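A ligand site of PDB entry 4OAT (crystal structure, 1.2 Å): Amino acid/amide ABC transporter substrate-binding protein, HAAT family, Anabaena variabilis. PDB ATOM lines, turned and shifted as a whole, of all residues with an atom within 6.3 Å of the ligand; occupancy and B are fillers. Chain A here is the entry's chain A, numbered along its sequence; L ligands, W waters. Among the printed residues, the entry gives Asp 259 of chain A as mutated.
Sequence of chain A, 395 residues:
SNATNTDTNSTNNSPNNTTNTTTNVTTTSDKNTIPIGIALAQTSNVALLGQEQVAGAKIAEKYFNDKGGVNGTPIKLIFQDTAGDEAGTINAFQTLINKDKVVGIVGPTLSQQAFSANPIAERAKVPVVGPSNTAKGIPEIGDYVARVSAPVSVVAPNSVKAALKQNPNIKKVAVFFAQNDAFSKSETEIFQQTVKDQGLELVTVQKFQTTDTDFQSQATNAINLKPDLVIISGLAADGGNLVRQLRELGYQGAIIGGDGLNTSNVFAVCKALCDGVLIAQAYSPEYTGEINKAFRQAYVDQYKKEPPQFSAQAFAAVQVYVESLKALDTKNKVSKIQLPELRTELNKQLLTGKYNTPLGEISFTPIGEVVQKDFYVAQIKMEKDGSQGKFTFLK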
ATOM      1  N   LEU A  49      26.607 -23.814  15.916  1.00  0.00           N
ATOM      2  CA  LEU A  49      27.493 -24.960  15.723  1.00  0.00           C
ATOM      3  C   LEU A  49      28.855 -24.694  16.356  1.00  0.00           C
ATOM      4  O   LEU A  49      29.419 -25.545  17.070  1.00  0.00           O
ATOM      5  CB  LEU A  49      27.656 -25.229  14.225  1.00  0.00           C
ATOM      6  CG  LEU A  49      26.334 -25.397  13.469  1.00  0.00           C
ATOM      7  CD1 LEU A  49      26.537 -25.305  11.965  1.00  0.00           C
ATOM      8  CD2 LEU A  49      25.677 -26.713  13.823  1.00  0.00           C
ATOM      9  N   GLY A  50      29.386 -23.500  16.133  1.00  0.00           N
ATOM     10  CA  GLY A  50      30.730 -23.178  16.595  1.00  0.00           C
ATOM     11  C   GLY A  50      30.930 -23.168  18.100  1.00  0.00           C
ATOM     12  O   GLY A  50      32.000 -23.510  18.583  1.00  0.00           O
ATOM     13  N   GLN A  53      32.082 -26.373  19.489  1.00  0.00           N
ATOM     14  CA  GLN A  53      33.481 -26.594  19.163  1.00  0.00           C
ATOM     15  C   GLN A  53      34.382 -25.818  20.130  1.00  0.00           C
ATOM     16  O   GLN A  53      35.365 -26.356  20.631  1.00  0.00           O
ATOM     17  CB  GLN A  53      33.742 -26.162  17.720  1.00  0.00           C
ATOM     18  CG  GLN A  53      32.974 -26.953  16.702  1.00  0.00           C
ATOM     19  CD  GLN A  53      33.227 -26.452  15.312  1.00  0.00           C
ATOM     20  OE1 GLN A  53      33.210 -25.234  15.069  1.00  0.00           O
ATOM     21  NE2 GLN A  53      33.495 -27.364  14.386  1.00  0.00           N
ATOM     22  N   THR A 109      34.733 -23.363  11.308  1.00  0.00           N
ATOM     23  CA  THR A 109      33.566 -24.161  11.641  1.00  0.00           C
ATOM     24  C   THR A 109      32.959 -24.834  10.400  1.00  0.00           C
ATOM     25  O   THR A 109      32.690 -26.028  10.402  1.00  0.00           O
ATOM     26  CB  THR A 109      32.520 -23.304  12.377  1.00  0.00           C
ATOM     27  OG1 THR A 109      33.080 -22.881  13.630  1.00  0.00           O
ATOM     28  CG2 THR A 109      31.193 -24.038  12.608  1.00  0.00           C
ATOM     29  N   LEU A 110      32.707 -24.050   9.354  1.00  0.00           N
ATOM     30  CA  LEU A 110      31.978 -24.559   8.175  1.00  0.00           C
ATOM     31  C   LEU A 110      32.876 -24.899   7.003  1.00  0.00           C
ATOM     32  O   LEU A 110      33.839 -24.173   6.709  1.00  0.00           O
ATOM     33  CB  LEU A 110      30.997 -23.496   7.679  1.00  0.00           C
ATOM     34  CG  LEU A 110      29.866 -23.142   8.624  1.00  0.00           C
ATOM     35  CD1 LEU A 110      29.021 -22.056   7.984  1.00  0.00           C
ATOM     36  CD2 LEU A 110      28.993 -24.358   8.986  1.00  0.00           C
ATOM     37  N   SER A 111      32.498 -25.953   6.274  1.00  0.00           N
ATOM     38  CA  SER A 111      33.123 -26.209   4.975  1.00  0.00           C
ATOM     39  C   SER A 111      33.059 -25.001   4.050  1.00  0.00           C
ATOM     40  O   SER A 111      34.023 -24.696   3.348  1.00  0.00           O
ATOM     41  CB  SER A 111      32.486 -27.417   4.299  1.00  0.00           C
ATOM     42  OG  SER A 111      32.747 -28.623   4.989  1.00  0.00           O
ATOM     43  N   GLN A 112      31.916 -24.311   4.059  1.00  0.00           N
ATOM     44  CA  GLN A 112      31.742 -23.113   3.226  1.00  0.00           C
ATOM     45  C   GLN A 112      32.884 -22.120   3.478  1.00  0.00           C
ATOM     46  O   GLN A 112      33.396 -21.495   2.551  1.00  0.00           O
ATOM     47  CB  GLN A 112      30.408 -22.462   3.553  1.00  0.00           C
ATOM     48  CG  GLN A 112      30.156 -21.152   2.799  1.00  0.00           C
ATOM     49  CD  GLN A 112      29.913 -21.353   1.322  1.00  0.00           C
ATOM     50  OE1 GLN A 112      29.392 -22.393   0.887  1.00  0.00           O
ATOM     51  NE2 GLN A 112      30.276 -20.353   0.531  1.00  0.00           N
ATOM     52  N   SER A 132      35.402 -30.281  12.093  1.00  0.00           N
ATOM     53  CA  SER A 132      34.074 -30.822  11.795  1.00  0.00           C
ATOM     54  C   SER A 132      33.656 -30.632  10.354  1.00  0.00           C
ATOM     55  O   SER A 132      32.502 -30.952  10.032  1.00  0.00           O
ATOM     56  CB  SER A 132      33.026 -30.172  12.702  1.00  0.00           C
ATOM     57  OG  SER A 132      33.428 -30.227  14.073  1.00  0.00           O
ATOM     58  N   ASN A 133      34.539 -30.089   9.513  1.00  0.00           N
ATOM     59  CA  ASN A 133      34.169 -29.812   8.129  1.00  0.00           C
ATOM     60  C   ASN A 133      34.218 -31.052   7.272  1.00  0.00           C
ATOM     61  O   ASN A 133      35.267 -31.674   7.114  1.00  0.00           O
ATOM     62  CB  ASN A 133      34.853 -28.571   7.541  1.00  0.00           C
ATOM     63  CG  ASN A 133      36.365 -28.531   7.686  1.00  0.00           C
ATOM     64  OD1 ASN A 133      36.933 -27.430   7.606  1.00  0.00           O
ATOM     65  ND2 ASN A 133      37.042 -29.678   7.841  1.00  0.00           N
ATOM     66  N   THR A 134      33.061 -31.418   6.742  1.00  0.00           N
ATOM     67  CA  THR A 134      32.882 -32.729   6.146  1.00  0.00           C
ATOM     68  C   THR A 134      32.541 -32.743   4.662  1.00  0.00           C
ATOM     69  O   THR A 134      32.281 -33.809   4.095  1.00  0.00           O
ATOM     70  CB  THR A 134      31.840 -33.552   6.930  1.00  0.00           C
ATOM     71  OG1 THR A 134      30.608 -32.820   6.976  1.00  0.00           O
ATOM     72  CG2 THR A 134      32.365 -33.826   8.368  1.00  0.00           C
ATOM     73  N   ALA A 135      32.577 -31.576   4.007  1.00  0.00           N
ATOM     74  CA  ALA A 135      32.344 -31.548   2.565  1.00  0.00           C
ATOM     75  C   ALA A 135      33.437 -32.311   1.813  1.00  0.00           C
ATOM     76  O   ALA A 135      34.606 -32.357   2.223  1.00  0.00           O
ATOM     77  CB  ALA A 135      32.280 -30.121   2.046  1.00  0.00           C
ATOM     78  N   ILE A 138      37.906 -31.115   1.033  1.00  0.00           N
ATOM     79  CA  ILE A 138      38.642 -30.212   1.916  1.00  0.00           C
ATOM     80  C   ILE A 138      40.136 -30.549   2.091  1.00  0.00           C
ATOM     81  O   ILE A 138      40.966 -29.663   1.925  1.00  0.00           O
ATOM     82  CB  ILE A 138      37.905 -29.966   3.231  1.00  0.00           C
ATOM     83  CG1 ILE A 138      36.566 -29.294   2.907  1.00  0.00           C
ATOM     84  CG2 ILE A 138      38.745 -29.082   4.141  1.00  0.00           C
ATOM     85  CD1 ILE A 138      35.806 -28.923   4.127  1.00  0.00           C
ATOM     86  N   VAL A 152      31.129 -36.544   4.414  1.00  0.00           N
ATOM     87  CA  VAL A 152      29.720 -36.870   4.241  1.00  0.00           C
ATOM     88  C   VAL A 152      29.481 -38.229   3.585  1.00  0.00           C
ATOM     89  O   VAL A 152      28.503 -38.891   3.897  1.00  0.00           O
ATOM     90  CB  VAL A 152      28.969 -35.761   3.461  1.00  0.00           C
ATOM     91  CG1 VAL A 152      28.860 -34.497   4.301  1.00  0.00           C
ATOM     92  CG2 VAL A 152      29.668 -35.466   2.139  1.00  0.00           C
ATOM     93  N   ASP A 181      25.130 -23.291   0.783  1.00  0.00           N
ATOM     94  CA  ASP A 181      26.121 -23.806   1.723  1.00  0.00           C
ATOM     95  C   ASP A 181      26.868 -25.011   1.153  1.00  0.00           C
ATOM     96  O   ASP A 181      26.250 -25.990   0.742  1.00  0.00           O
ATOM     97  CB  ASP A 181      25.463 -24.158   3.049  1.00  0.00           C
ATOM     98  CG  ASP A 181      26.430 -24.774   4.033  1.00  0.00           C
ATOM     99  OD1 ASP A 181      27.251 -24.009   4.605  1.00  0.00           O
ATOM    100  OD2 ASP A 181      26.413 -25.999   4.210  1.00  0.00           O
ATOM    101  N   PHE A 183      28.832 -27.426   2.378  1.00  0.00           N
ATOM    102  CA  PHE A 183      28.641 -28.716   3.002  1.00  0.00           C
ATOM    103  C   PHE A 183      27.250 -29.285   2.730  1.00  0.00           C
ATOM    104  O   PHE A 183      27.111 -30.481   2.469  1.00  0.00           O
ATOM    105  CB  PHE A 183      28.914 -28.647   4.505  1.00  0.00           C
ATOM    106  CG  PHE A 183      28.000 -29.491   5.335  1.00  0.00           C
ATOM    107  CD1 PHE A 183      28.244 -30.836   5.546  1.00  0.00           C
ATOM    108  CD2 PHE A 183      26.849 -28.937   5.877  1.00  0.00           C
ATOM    109  CE1 PHE A 183      27.365 -31.608   6.317  1.00  0.00           C
ATOM    110  CE2 PHE A 183      25.971 -29.692   6.634  1.00  0.00           C
ATOM    111  CZ  PHE A 183      26.227 -31.030   6.847  1.00  0.00           C
ATOM    112  N   SER A 184      26.224 -28.434   2.758  1.00  0.00           N
ATOM    113  CA  SER A 184      24.858 -28.918   2.534  1.00  0.00           C
ATOM    114  C   SER A 184      24.699 -29.489   1.136  1.00  0.00           C
ATOM    115  O   SER A 184      24.049 -30.507   0.942  1.00  0.00           O
ATOM    116  CB  SER A 184      23.840 -27.798   2.769  1.00  0.00           C
ATOM    117  OG  SER A 184      23.863 -27.351   4.123  1.00  0.00           O
ATOM    118  N   GLY A 234      20.831 -28.779   5.998  1.00  0.00           N
ATOM    119  CA  GLY A 234      21.047 -27.359   6.211  1.00  0.00           C
ATOM    120  C   GLY A 234      21.869 -27.174   7.457  1.00  0.00           C
ATOM    121  O   GLY A 234      22.544 -28.105   7.895  1.00  0.00           O
ATOM    122  N   LEU A 235      21.830 -25.971   8.001  1.00  0.00           N
ATOM    123  CA  LEU A 235      22.455 -25.714   9.284  1.00  0.00           C
ATOM    124  C   LEU A 235      21.401 -25.687  10.396  1.00  0.00           C
ATOM    125  O   LEU A 235      20.308 -26.242  10.216  1.00  0.00           O
ATOM    126  CB  LEU A 235      23.346 -24.467   9.232  1.00  0.00           C
ATOM    127  CG  LEU A 235      24.392 -24.517   8.100  1.00  0.00           C
ATOM    128  CD1 LEU A 235      25.233 -23.252   8.092  1.00  0.00           C
ATOM    129  CD2 LEU A 235      25.276 -25.758   8.184  1.00  0.00           C
ATOM    130  N   ASP A 259      24.276 -33.171   9.280  1.00  0.00           N
ATOM    131  CA  ASP A 259      25.198 -32.788  10.343  1.00  0.00           C
ATOM    132  C   ASP A 259      24.949 -31.349  10.834  1.00  0.00           C
ATOM    133  O   ASP A 259      25.285 -31.024  11.985  1.00  0.00           O
ATOM    134  CB  ASP A 259      26.639 -32.956   9.840  1.00  0.00           C
ATOM    135  CG  ASP A 259      27.666 -33.032  10.962  1.00  0.00           C
ATOM    136  OD1 ASP A 259      27.471 -33.839  11.902  1.00  0.00           O
ATOM    137  OD2 ASP A 259      28.687 -32.299  10.877  1.00  0.00           O
ATOM    138  N   GLY A 260      24.396 -30.491   9.990  1.00  0.00           N
ATOM    139  CA  GLY A 260      24.139 -29.128  10.403  1.00  0.00           C
ATOM    140  C   GLY A 260      23.016 -28.995  11.414  1.00  0.00           C
ATOM    141  O   GLY A 260      22.876 -27.934  12.012  1.00  0.00           O
ATOM    142  N   LEU A 261      22.240 -30.057  11.617  1.00  0.00           N
ATOM    143  CA  LEU A 261      21.185 -30.059  12.639  1.00  0.00           C
ATOM    144  C   LEU A 261      21.667 -30.766  13.909  1.00  0.00           C
ATOM    145  O   LEU A 261      20.887 -30.933  14.855  1.00  0.00           O
ATOM    146  CB  LEU A 261      19.924 -30.751  12.125  1.00  0.00           C
ATOM    147  CG  LEU A 261      19.058 -29.939  11.144  1.00  0.00           C
ATOM    148  CD1 LEU A 261      19.705 -29.849   9.756  1.00  0.00           C
ATOM    149  CD2 LEU A 261      17.653 -30.525  11.053  1.00  0.00           C
ATOM    150  N   GLN A 309      29.001 -34.263  19.566  1.00  0.00           N
ATOM    151  CA  GLN A 309      30.000 -34.538  18.546  1.00  0.00           C
ATOM    152  C   GLN A 309      30.944 -33.360  18.282  1.00  0.00           C
ATOM    153  O   GLN A 309      32.157 -33.556  18.225  1.00  0.00           O
ATOM    154  CB  GLN A 309      29.289 -34.899  17.245  1.00  0.00           C
ATOM    155  CG  GLN A 309      30.235 -35.127  16.096  1.00  0.00           C
ATOM    156  CD  GLN A 309      29.460 -35.251  14.808  1.00  0.00           C
ATOM    157  OE1 GLN A 309      28.846 -36.280  14.539  1.00  0.00           O
ATOM    158  NE2 GLN A 309      29.443 -34.176  14.006  1.00  0.00           N
ATOM    159  N   PHE A 310      30.407 -32.159  18.096  1.00  0.00           N
ATOM    160  CA  PHE A 310      31.260 -31.032  17.718  1.00  0.00           C
ATOM    161  C   PHE A 310      32.287 -30.709  18.800  1.00  0.00           C
ATOM    162  O   PHE A 310      33.395 -30.273  18.486  1.00  0.00           O
ATOM    163  CB  PHE A 310      30.452 -29.780  17.402  1.00  0.00           C
ATOM    164  CG  PHE A 310      29.533 -29.926  16.204  1.00  0.00           C
ATOM    165  CD1 PHE A 310      29.936 -30.586  15.049  1.00  0.00           C
ATOM    166  CD2 PHE A 310      28.251 -29.394  16.252  1.00  0.00           C
ATOM    167  CE1 PHE A 310      29.056 -30.690  13.965  1.00  0.00           C
ATOM    168  CE2 PHE A 310      27.392 -29.511  15.183  1.00  0.00           C
ATOM    169  CZ  PHE A 310      27.782 -30.157  14.058  1.00  0.00           C
ATOM    170  N   GLN A 313      35.055 -33.404  18.536  1.00  0.00           N
ATOM    171  CA  GLN A 313      35.872 -33.158  17.358  1.00  0.00           C
ATOM    172  C   GLN A 313      36.878 -32.033  17.570  1.00  0.00           C
ATOM    173  O   GLN A 313      38.051 -32.143  17.182  1.00  0.00           O
ATOM    174  CB  GLN A 313      34.984 -32.845  16.165  1.00  0.00           C
ATOM    175  CG  GLN A 313      34.238 -34.054  15.640  1.00  0.00           C
ATOM    176  CD  GLN A 313      33.173 -33.686  14.619  1.00  0.00           C
ATOM    177  OE1 GLN A 313      32.520 -32.644  14.723  1.00  0.00           O
ATOM    178  NE2 GLN A 313      32.983 -34.556  13.628  1.00  0.00           N
HETATM  179  N1  LIG L   1      29.880 -30.631   8.855  1.00  0.00           N
HETATM  180  C1  LIG L   1      29.361 -29.312   8.512  1.00  0.00           C
HETATM  181  C2  LIG L   1      30.311 -28.593   7.558  1.00  0.00           C
HETATM  182  O1  LIG L   1      31.225 -29.256   7.030  1.00  0.00           O
HETATM  183  C3  LIG L   1      29.034 -28.458   9.769  1.00  0.00           C
HETATM  184  C4  LIG L   1      30.211 -28.456  10.772  1.00  0.00           C
HETATM  185  C5  LIG L   1      27.764 -28.981  10.443  1.00  0.00           C
HETATM  186  C6  LIG L   1      29.987 -27.541  11.949  1.00  0.00           C
HETATM  187  O2  LIG L   1      30.165 -27.388   7.297  1.00  0.00           O
HETATM  188  O   HOH W   1      29.519 -25.401   5.154  1.00  0.00           O
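Leu 49 touches the ligand (CB to C6, 3.99 Å). O of Thr 109 touches C6 of the ligand, at 3.5 Å. Leu 110 touches the ligand. Asn 133 touches the ligand (CA to O1, 3.2 Å). Phe 183 touches the ligand (CB to O2, 3.3 Å). CA of Gly 260 touches C5 of the ligand, at 3.6 Å. Phe 310 touches the ligand (CZ to C5, 3.8 Å). Hydrophobic or aromatic side chains within 4 Å of the ligand: Leu 49, Leu 110, Phe 183 and Phe 310. Of the 24 residues printed, 11 come within 4 Å of the ligand. The nearest printed residue that does not touch the ligand is Ala 135 (4.04 Å).
OG of Ser 132 lies within hydrogen-bond range of OE1 of Gln 313 (2.7 Å). The backbone NH (N) of Phe 183 lies close to the side-chain carboxylate (OD2) of Asp 181 (3.4 Å). The side-chain hydroxyl (OG1) of Thr 109 is in hydrogen-bond range of the side-chain amide oxygen (OE1) of Gln 53. The side-chain carboxylate of Asp 259 sits at hydrogen-bond distance from the side-chain amide nitrogen of Gln 309. O of Thr 134 lies within hydrogen-bond range of N of Val 152. N of Ala 135 sits at hydrogen-bond distance from OG of Ser 111 (3.1 Å). The side-chain amide nitrogen (NE2) of Gln 53 lies within hydrogen-bond range of the side-chain hydroxyl (OG) of Ser 132. N of Thr 134 lies within hydrogen-bond range of OG of Ser 111 (3.3 Å).
Water W1 lies within hydrogen-bond range of OD1 of Asp 181 (2.7 Å), N of Gln 112 (2.9 Å), O2 of the ligand (3.0 Å) and N of Ser 111 (3.2 Å).
The side-chain hydroxyl (OG) of Ser 111 lies within hydrogen-bond range of an oxygen (O1) of the ligand (2.6 Å). The backbone NH (N) of Ser 111 is in hydrogen-bond range of an oxygen (O2) of the ligand. N1 of the ligand lies within salt-bridge range of OD2 of Asp 259, 2.9 Å away. The side-chain hydroxyl (OG1) of Thr 134 lies within hydrogen-bond range of a nitrogen (N1) of the ligand (3.0 Å). The backbone carbonyl oxygen of Ser 132 sits at hydrogen-bond distance from a nitrogen (N1) of the ligand, 2.9 Å away. The backbone NH of Thr 134 is in hydrogen-bond range of an oxygen (O1) of the ligand (2.9 Å).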
